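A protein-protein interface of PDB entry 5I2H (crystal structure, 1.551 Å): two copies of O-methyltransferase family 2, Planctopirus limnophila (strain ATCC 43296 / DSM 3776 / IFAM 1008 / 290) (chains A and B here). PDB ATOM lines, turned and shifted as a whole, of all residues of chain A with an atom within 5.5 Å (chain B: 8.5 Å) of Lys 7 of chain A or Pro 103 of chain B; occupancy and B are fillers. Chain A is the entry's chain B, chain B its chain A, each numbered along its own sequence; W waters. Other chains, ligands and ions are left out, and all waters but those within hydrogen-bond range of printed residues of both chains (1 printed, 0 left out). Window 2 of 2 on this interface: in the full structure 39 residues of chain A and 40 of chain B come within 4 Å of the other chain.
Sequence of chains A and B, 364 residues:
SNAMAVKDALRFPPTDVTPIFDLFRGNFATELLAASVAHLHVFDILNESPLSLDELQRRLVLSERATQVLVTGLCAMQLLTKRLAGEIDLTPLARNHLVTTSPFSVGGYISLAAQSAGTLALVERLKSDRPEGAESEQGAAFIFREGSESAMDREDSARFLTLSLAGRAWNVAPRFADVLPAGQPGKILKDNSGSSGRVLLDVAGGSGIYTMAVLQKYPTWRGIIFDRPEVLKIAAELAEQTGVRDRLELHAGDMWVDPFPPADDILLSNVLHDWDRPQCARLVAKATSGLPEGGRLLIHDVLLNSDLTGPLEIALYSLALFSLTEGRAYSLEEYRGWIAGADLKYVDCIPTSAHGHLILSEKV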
ATOM      1  N   ALA A   5     -21.762   8.722 -37.424  1.00  0.00           N
ATOM      2  CA  ALA A   5     -21.697   8.230 -36.046  1.00  0.00           C
ATOM      3  C   ALA A   5     -23.070   8.304 -35.391  1.00  0.00           C
ATOM      4  O   ALA A   5     -23.827   9.254 -35.617  1.00  0.00           O
ATOM      5  CB  ALA A   5     -20.689   9.046 -35.222  1.00  0.00           C
ATOM      6  N   VAL A   6     -23.410   7.292 -34.592  1.00  0.00           N
ATOM      7  CA  VAL A   6     -24.704   7.282 -33.916  1.00  0.00           C
ATOM      8  C   VAL A   6     -24.480   7.089 -32.417  1.00  0.00           C
ATOM      9  O   VAL A   6     -23.876   6.095 -31.988  1.00  0.00           O
ATOM     10  CB  VAL A   6     -25.653   6.213 -34.484  1.00  0.00           C
ATOM     11  CG1 VAL A   6     -26.954   6.224 -33.729  1.00  0.00           C
ATOM     12  CG2 VAL A   6     -25.929   6.470 -35.964  1.00  0.00           C
ATOM     13  N   LYS A   7     -24.953   8.047 -31.629  1.00  0.00           N
ATOM     14  CA  LYS A   7     -24.925   7.934 -30.171  1.00  0.00           C
ATOM     15  C   LYS A   7     -25.925   6.890 -29.694  1.00  0.00           C
ATOM     16  O   LYS A   7     -27.111   6.943 -30.044  1.00  0.00           O
ATOM     17  CB  LYS A   7     -25.235   9.297 -29.542  1.00  0.00           C
ATOM     18  CG  LYS A   7     -25.146   9.332 -28.016  1.00  0.00           C
ATOM     19  CD  LYS A   7     -25.338  10.761 -27.505  1.00  0.00           C
ATOM     20  CE  LYS A   7     -25.320  10.818 -25.986  1.00  0.00           C
ATOM     21  NZ  LYS A   7     -24.006  10.320 -25.453  1.00  0.00           N
ATOM     22  N   ASP A   8     -25.457   5.940 -28.884  1.00  0.00           N
ATOM     23  CA  ASP A   8     -26.349   4.888 -28.409  1.00  0.00           C
ATOM     24  C   ASP A   8     -27.137   5.385 -27.206  1.00  0.00           C
ATOM     25  O   ASP A   8     -26.568   5.950 -26.269  1.00  0.00           O
ATOM     26  CB  ASP A   8     -25.586   3.620 -28.045  1.00  0.00           C
ATOM     27  CG  ASP A   8     -26.461   2.670 -27.260  1.00  0.00           C
ATOM     28  OD1 ASP A   8     -27.412   2.105 -27.817  1.00  0.00           O
ATOM     29  OD2 ASP A   8     -26.269   2.579 -26.035  1.00  0.00           O
ATOM     30  N   ALA A   9     -28.452   5.186 -27.232  1.00  0.00           N
ATOM     31  CA  ALA A   9     -29.300   5.577 -26.118  1.00  0.00           C
ATOM     32  C   ALA A   9     -29.901   4.358 -25.427  1.00  0.00           C
ATOM     33  O   ALA A   9     -30.709   4.503 -24.499  1.00  0.00           O
ATOM     34  CB  ALA A   9     -30.397   6.536 -26.608  1.00  0.00           C
ATOM     35  N   GLY A 167     -28.436  14.766 -17.968  1.00  0.00           N
ATOM     36  CA  GLY A 167     -27.588  13.693 -17.487  1.00  0.00           C
ATOM     37  C   GLY A 167     -28.384  12.610 -16.782  1.00  0.00           C
ATOM     38  O   GLY A 167     -28.107  11.416 -16.940  1.00  0.00           O
ATOM     39  N   TRP A 170     -29.948  10.477 -19.541  1.00  0.00           N
ATOM     40  CA  TRP A 170     -29.059   9.512 -20.196  1.00  0.00           C
ATOM     41  C   TRP A 170     -28.884   8.268 -19.329  1.00  0.00           C
ATOM     42  O   TRP A 170     -28.695   7.180 -19.855  1.00  0.00           O
ATOM     43  CB  TRP A 170     -27.674  10.110 -20.502  1.00  0.00           C
ATOM     44  CG  TRP A 170     -27.691  11.161 -21.586  1.00  0.00           C
ATOM     45  CD1 TRP A 170     -27.328  12.490 -21.455  1.00  0.00           C
ATOM     46  CD2 TRP A 170     -28.087  10.989 -22.971  1.00  0.00           C
ATOM     47  NE1 TRP A 170     -27.517  13.141 -22.655  1.00  0.00           N
ATOM     48  CE2 TRP A 170     -27.959  12.247 -23.600  1.00  0.00           C
ATOM     49  CE3 TRP A 170     -28.562   9.896 -23.729  1.00  0.00           C
ATOM     50  CZ2 TRP A 170     -28.275  12.452 -24.956  1.00  0.00           C
ATOM     51  CZ3 TRP A 170     -28.867  10.096 -25.087  1.00  0.00           C
ATOM     52  CH2 TRP A 170     -28.711  11.371 -25.685  1.00  0.00           C
ATOM     53  N   ASN A 171     -28.924   8.418 -17.999  1.00  0.00           N
ATOM     54  CA  ASN A 171     -28.827   7.255 -17.120  1.00  0.00           C
ATOM     55  C   ASN A 171     -30.096   6.405 -17.092  1.00  0.00           C
ATOM     56  O   ASN A 171     -30.009   5.166 -16.906  1.00  0.00           O
ATOM     57  CB  ASN A 171     -28.475   7.708 -15.697  1.00  0.00           C
ATOM     58  CG  ASN A 171     -26.997   8.024 -15.562  1.00  0.00           C
ATOM     59  OD1 ASN A 171     -26.207   7.129 -15.259  1.00  0.00           O
ATOM     60  ND2 ASN A 171     -26.600   9.296 -15.842  1.00  0.00           N
ATOM     61  N   GLN A 216     -34.964   4.511 -30.831  1.00  0.00           N
ATOM     62  CA  GLN A 216     -33.928   3.540 -31.191  1.00  0.00           C
ATOM     63  C   GLN A 216     -34.399   2.105 -30.957  1.00  0.00           C
ATOM     64  O   GLN A 216     -34.041   1.195 -31.722  1.00  0.00           O
ATOM     65  CB  GLN A 216     -32.628   3.812 -30.418  1.00  0.00           C
ATOM     66  CG  GLN A 216     -31.905   5.076 -30.858  1.00  0.00           C
ATOM     67  CD  GLN A 216     -30.522   5.187 -30.242  1.00  0.00           C
ATOM     68  OE1 GLN A 216     -30.160   4.436 -29.331  1.00  0.00           O
ATOM     69  NE2 GLN A 216     -29.732   6.128 -30.740  1.00  0.00           N
ATOM     70  N   GLN A 241     -27.511  13.567 -32.957  1.00  0.00           N
ATOM     71  CA  GLN A 241     -26.484  12.683 -32.419  1.00  0.00           C
ATOM     72  C   GLN A 241     -26.970  11.240 -32.357  1.00  0.00           C
ATOM     73  O   GLN A 241     -26.205  10.308 -32.658  1.00  0.00           O
ATOM     74  CB  GLN A 241     -26.065  13.151 -31.020  1.00  0.00           C
ATOM     75  CG  GLN A 241     -25.270  14.428 -30.994  1.00  0.00           C
ATOM     76  CD  GLN A 241     -24.891  14.806 -29.566  1.00  0.00           C
ATOM     77  OE1 GLN A 241     -24.786  13.931 -28.702  1.00  0.00           O
ATOM     78  NE2 GLN A 241     -24.722  16.098 -29.301  1.00  0.00           N
ATOM     79  N   THR A 242     -28.240  11.034 -31.957  1.00  0.00           N
ATOM     80  CA  THR A 242     -28.761   9.695 -31.758  1.00  0.00           C
ATOM     81  C   THR A 242     -29.340   9.112 -33.040  1.00  0.00           C
ATOM     82  O   THR A 242     -29.846   7.985 -33.021  1.00  0.00           O
ATOM     83  CB  THR A 242     -29.826   9.680 -30.646  1.00  0.00           C
ATOM     84  OG1 THR A 242     -30.869  10.617 -30.955  1.00  0.00           O
ATOM     85  CG2 THR A 242     -29.184  10.055 -29.292  1.00  0.00           C
ATOM     86  N   GLY A 243     -29.279   9.846 -34.152  1.00  0.00           N
ATOM     87  CA  GLY A 243     -29.681   9.300 -35.437  1.00  0.00           C
ATOM     88  C   GLY A 243     -31.167   9.086 -35.599  1.00  0.00           C
ATOM     89  O   GLY A 243     -31.581   8.287 -36.449  1.00  0.00           O
ATOM     90  N   ARG B  95     -16.178   7.802 -11.896  1.00  0.00           N
ATOM     91  CA  ARG B  95     -15.677   7.909 -13.261  1.00  0.00           C
ATOM     92  C   ARG B  95     -16.830   7.977 -14.263  1.00  0.00           C
ATOM     93  O   ARG B  95     -16.764   8.711 -15.268  1.00  0.00           O
ATOM     94  CB  ARG B  95     -14.742   6.740 -13.563  1.00  0.00           C
ATOM     95  CG  ARG B  95     -13.863   6.971 -14.810  1.00  0.00           C
ATOM     96  CD  ARG B  95     -12.851   5.858 -15.074  1.00  0.00           C
ATOM     97  NE  ARG B  95     -12.094   5.423 -13.885  1.00  0.00           N
ATOM     98  CZ  ARG B  95     -10.920   5.919 -13.469  1.00  0.00           C
ATOM     99  NH1 ARG B  95     -10.358   6.956 -14.077  1.00  0.00           N
ATOM    100  NH2 ARG B  95     -10.336   5.396 -12.382  1.00  0.00           N
ATOM    101  N   ASN B  96     -17.900   7.220 -14.006  1.00  0.00           N
ATOM    102  CA  ASN B  96     -19.026   7.175 -14.933  1.00  0.00           C
ATOM    103  C   ASN B  96     -19.972   8.350 -14.767  1.00  0.00           C
ATOM    104  O   ASN B  96     -20.658   8.723 -15.724  1.00  0.00           O
ATOM    105  CB  ASN B  96     -19.807   5.871 -14.750  1.00  0.00           C
ATOM    106  CG  ASN B  96     -18.977   4.665 -15.139  1.00  0.00           C
ATOM    107  OD1 ASN B  96     -18.133   4.773 -16.013  1.00  0.00           O
ATOM    108  ND2 ASN B  96     -19.191   3.529 -14.479  1.00  0.00           N
ATOM    109  N   HIS B  97     -20.072   8.915 -13.570  1.00  0.00           N
ATOM    110  CA  HIS B  97     -21.145   9.864 -13.324  1.00  0.00           C
ATOM    111  C   HIS B  97     -20.691  11.257 -12.912  1.00  0.00           C
ATOM    112  O   HIS B  97     -21.524  12.164 -12.892  1.00  0.00           O
ATOM    113  CB  HIS B  97     -22.109   9.282 -12.275  1.00  0.00           C
ATOM    114  CG  HIS B  97     -22.591   7.919 -12.653  1.00  0.00           C
ATOM    115  ND1 HIS B  97     -23.302   7.690 -13.809  1.00  0.00           N
ATOM    116  CD2 HIS B  97     -22.448   6.712 -12.048  1.00  0.00           C
ATOM    117  CE1 HIS B  97     -23.568   6.395 -13.905  1.00  0.00           C
ATOM    118  NE2 HIS B  97     -23.060   5.780 -12.853  1.00  0.00           N
ATOM    119  N   VAL B  99     -17.473  12.683 -14.061  1.00  0.00           N
ATOM    120  CA  VAL B  99     -16.527  13.200 -15.052  1.00  0.00           C
ATOM    121  C   VAL B  99     -17.337  13.828 -16.179  1.00  0.00           C
ATOM    122  O   VAL B  99     -18.309  13.228 -16.669  1.00  0.00           O
ATOM    123  CB  VAL B  99     -15.613  12.072 -15.557  1.00  0.00           C
ATOM    124  CG1 VAL B  99     -14.757  12.539 -16.729  1.00  0.00           C
ATOM    125  CG2 VAL B  99     -14.703  11.574 -14.435  1.00  0.00           C
ATOM    126  N   THR B 100     -16.950  15.049 -16.597  1.00  0.00           N
ATOM    127  CA  THR B 100     -17.796  15.854 -17.491  1.00  0.00           C
ATOM    128  C   THR B 100     -17.945  15.266 -18.895  1.00  0.00           C
ATOM    129  O   THR B 100     -18.918  15.593 -19.587  1.00  0.00           O
ATOM    130  CB  THR B 100     -17.281  17.308 -17.623  1.00  0.00           C
ATOM    131  OG1 THR B 100     -15.946  17.349 -18.170  1.00  0.00           O
ATOM    132  CG2 THR B 100     -17.334  18.040 -16.280  1.00  0.00           C
ATOM    133  N   THR B 101     -17.011  14.436 -19.349  1.00  0.00           N
ATOM    134  CA  THR B 101     -17.097  13.878 -20.691  1.00  0.00           C
ATOM    135  C   THR B 101     -17.650  12.460 -20.689  1.00  0.00           C
ATOM    136  O   THR B 101     -17.727  11.827 -21.747  1.00  0.00           O
ATOM    137  CB  THR B 101     -15.732  13.920 -21.384  1.00  0.00           C
ATOM    138  OG1 THR B 101     -14.753  13.417 -20.484  1.00  0.00           O
ATOM    139  CG2 THR B 101     -15.359  15.360 -21.719  1.00  0.00           C
ATOM    140  N   SER B 102     -18.071  11.973 -19.548  1.00  0.00           N
ATOM    141  CA  SER B 102     -18.742  10.687 -19.530  1.00  0.00           C
ATOM    142  C   SER B 102     -20.169  10.825 -20.055  1.00  0.00           C
ATOM    143  O   SER B 102     -20.888  11.753 -19.672  1.00  0.00           O
ATOM    144  CB  SER B 102     -18.809  10.114 -18.107  1.00  0.00           C
ATOM    145  OG  SER B 102     -19.632   8.940 -18.108  1.00  0.00           O
ATOM    146  N   PRO B 103     -20.630   9.894 -20.894  1.00  0.00           N
ATOM    147  CA  PRO B 103     -22.001  10.022 -21.391  1.00  0.00           C
ATOM    148  C   PRO B 103     -23.017   9.864 -20.289  1.00  0.00           C
ATOM    149  O   PRO B 103     -24.159  10.302 -20.457  1.00  0.00           O
ATOM    150  CB  PRO B 103     -22.112   8.929 -22.462  1.00  0.00           C
ATOM    151  CG  PRO B 103     -20.916   8.068 -22.293  1.00  0.00           C
ATOM    152  CD  PRO B 103     -19.867   8.828 -21.563  1.00  0.00           C
ATOM    153  N   PHE B 104     -22.635   9.295 -19.143  1.00  0.00           N
ATOM    154  CA  PHE B 104     -23.557   9.135 -18.024  1.00  0.00           C
ATOM    155  C   PHE B 104     -23.289  10.136 -16.908  1.00  0.00           C
ATOM    156  O   PHE B 104     -23.738   9.945 -15.762  1.00  0.00           O
ATOM    157  CB  PHE B 104     -23.497   7.706 -17.504  1.00  0.00           C
ATOM    158  CG  PHE B 104     -23.886   6.687 -18.544  1.00  0.00           C
ATOM    159  CD1 PHE B 104     -25.198   6.643 -19.007  1.00  0.00           C
ATOM    160  CD2 PHE B 104     -22.931   5.834 -19.117  1.00  0.00           C
ATOM    161  CE1 PHE B 104     -25.597   5.690 -19.961  1.00  0.00           C
ATOM    162  CE2 PHE B 104     -23.307   4.893 -20.081  1.00  0.00           C
ATOM    163  CZ  PHE B 104     -24.635   4.828 -20.519  1.00  0.00           C
ATOM    164  N   SER B 105     -22.580  11.206 -17.222  1.00  0.00           N
ATOM    165  CA  SER B 105     -22.308  12.224 -16.219  1.00  0.00           C
ATOM    166  C   SER B 105     -23.592  12.880 -15.709  1.00  0.00           C
ATOM    167  O   SER B 105     -24.516  13.170 -16.476  1.00  0.00           O
ATOM    168  CB  SER B 105     -21.403  13.302 -16.811  1.00  0.00           C
ATOM    169  OG  SER B 105     -21.209  14.289 -15.806  1.00  0.00           O
ATOM    170  N   VAL B 106     -23.644  13.124 -14.397  1.00  0.00           N
ATOM    171  CA  VAL B 106     -24.662  13.984 -13.833  1.00  0.00           C
ATOM    172  C   VAL B 106     -24.029  15.209 -13.176  1.00  0.00           C
ATOM    173  O   VAL B 106     -24.626  15.822 -12.295  1.00  0.00           O
ATOM    174  CB  VAL B 106     -25.564  13.219 -12.844  1.00  0.00           C
ATOM    175  CG1 VAL B 106     -26.293  12.084 -13.594  1.00  0.00           C
ATOM    176  CG2 VAL B 106     -24.753  12.693 -11.661  1.00  0.00           C
HETATM  177  O   HOH W   1     -24.356  11.621 -22.987  1.00  0.00           O
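Of chain B, only Pro 103 (3.8 Å) comes within 4 Å of Lys 7 of chain A.
Of the printed residues of chain B, Gly 167 of chain A touches Ser 105 and Val 106.
Of the printed residues of chain B, Trp 170 of chain A touches Pro 103 (3.5 Å) and Phe 104 (3.4 Å).
Gln 216 of chain A touches none of the printed residues of chain B.
Printed residues of chain A within 4 Å of His 97 of chain B: Asn 171 (3.1 Å).
Pro 103 of chain B touches just these residues of chain A: Lys 7 and Trp 170.
Of the printed residues of chain A, Phe 104 of chain B touches Trp 170 and Asn 171.
Of the printed residues of chain A, Ser 105 of chain B touches Gly 167 (3.3 Å).
The nearest residue of chain B that does not touch Lys 7 of chain A is Phe 104 of chain B (6.5 Å).
The nearest residue of chain A that does not touch Pro 103 of chain B is Asn 171 of chain A (5.3 Å).
The nearest printed residue of chain A that does not touch His 97 of chain B is Gly 167 of chain A (6.8 Å).
Of the 11 printed residues of chain B, 5 touch a printed residue of chain A.
Of the 12 printed residues of chain A, 4 touch a printed residue of chain B.
Printed residues of chain A that touch a printed residue of chain B: Lys 7, Gly 167, Trp 170 and Asn 171.
Hydrophobic or aromatic side chains of chain A that line the printed part of chain B: Trp 170.
Along chain A the printed residues that touch a printed residue of chain B span positions 7 to 171.
Among the printed residues, 8 pairs touch across the chains.
The side-chain amide nitrogen of Asn 171 of chain A lies within hydrogen-bond range of the backbone carbonyl oxygen of Phe 104 of chain B (2.9 Å).
A ring nitrogen (ND1) of His 97 of chain B lies close to the side-chain amide oxygen (OD1) of Asn 171 of chain A (3.3 Å).
O of His 97 of chain B is in hydrogen-bond range of N of Val 106 of chain B, at 2.8 Å.
The backbone carbonyl oxygen (O) of Val 99 of chain B lies close to the side-chain hydroxyl (OG) of Ser 105 of chain B, 3.2 Å away.
The backbone carbonyl oxygen (O) of Gly 167 of chain A is in hydrogen-bond range of the side-chain amide nitrogen (ND2) of Asn 171 of chain A.
O of Asn 96 of chain B is in hydrogen-bond range of N of Ser 105 of chain B (3.5 Å).
The backbone NH (N) of Lys 7 of chain A sits at hydrogen-bond distance from the backbone carbonyl oxygen (O) of Gln 241 of chain A.
O of Lys 7 of chain A is in hydrogen-bond range of NE2 of Gln 216 of chain A, 2.8 Å away.
No position is printed for both chains.
Of the 8 pairs that touch across the chains among the printed residues, none has its exchanged pair printed and touching as well.
Water W1 lies within hydrogen-bond range of the side-chain amino group of Lys 7 of chain A (2.8 Å) and the backbone carbonyl oxygen of Pro 103 of chain B (2.9 Å).
Among the printed residues, pairs that only touch across the chains: Gly 167 of chain A with Ser 105 of chain B, Trp 170 of chain A with Phe 104 of chain B, Trp 170 of chain A with Pro 103 of chain B, Asn 171 of chain A with Val 106 of chain B, Lys 7 of chain A with Pro 103 of chain B and Gly 167 of chain A with Val 106 of chain B.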
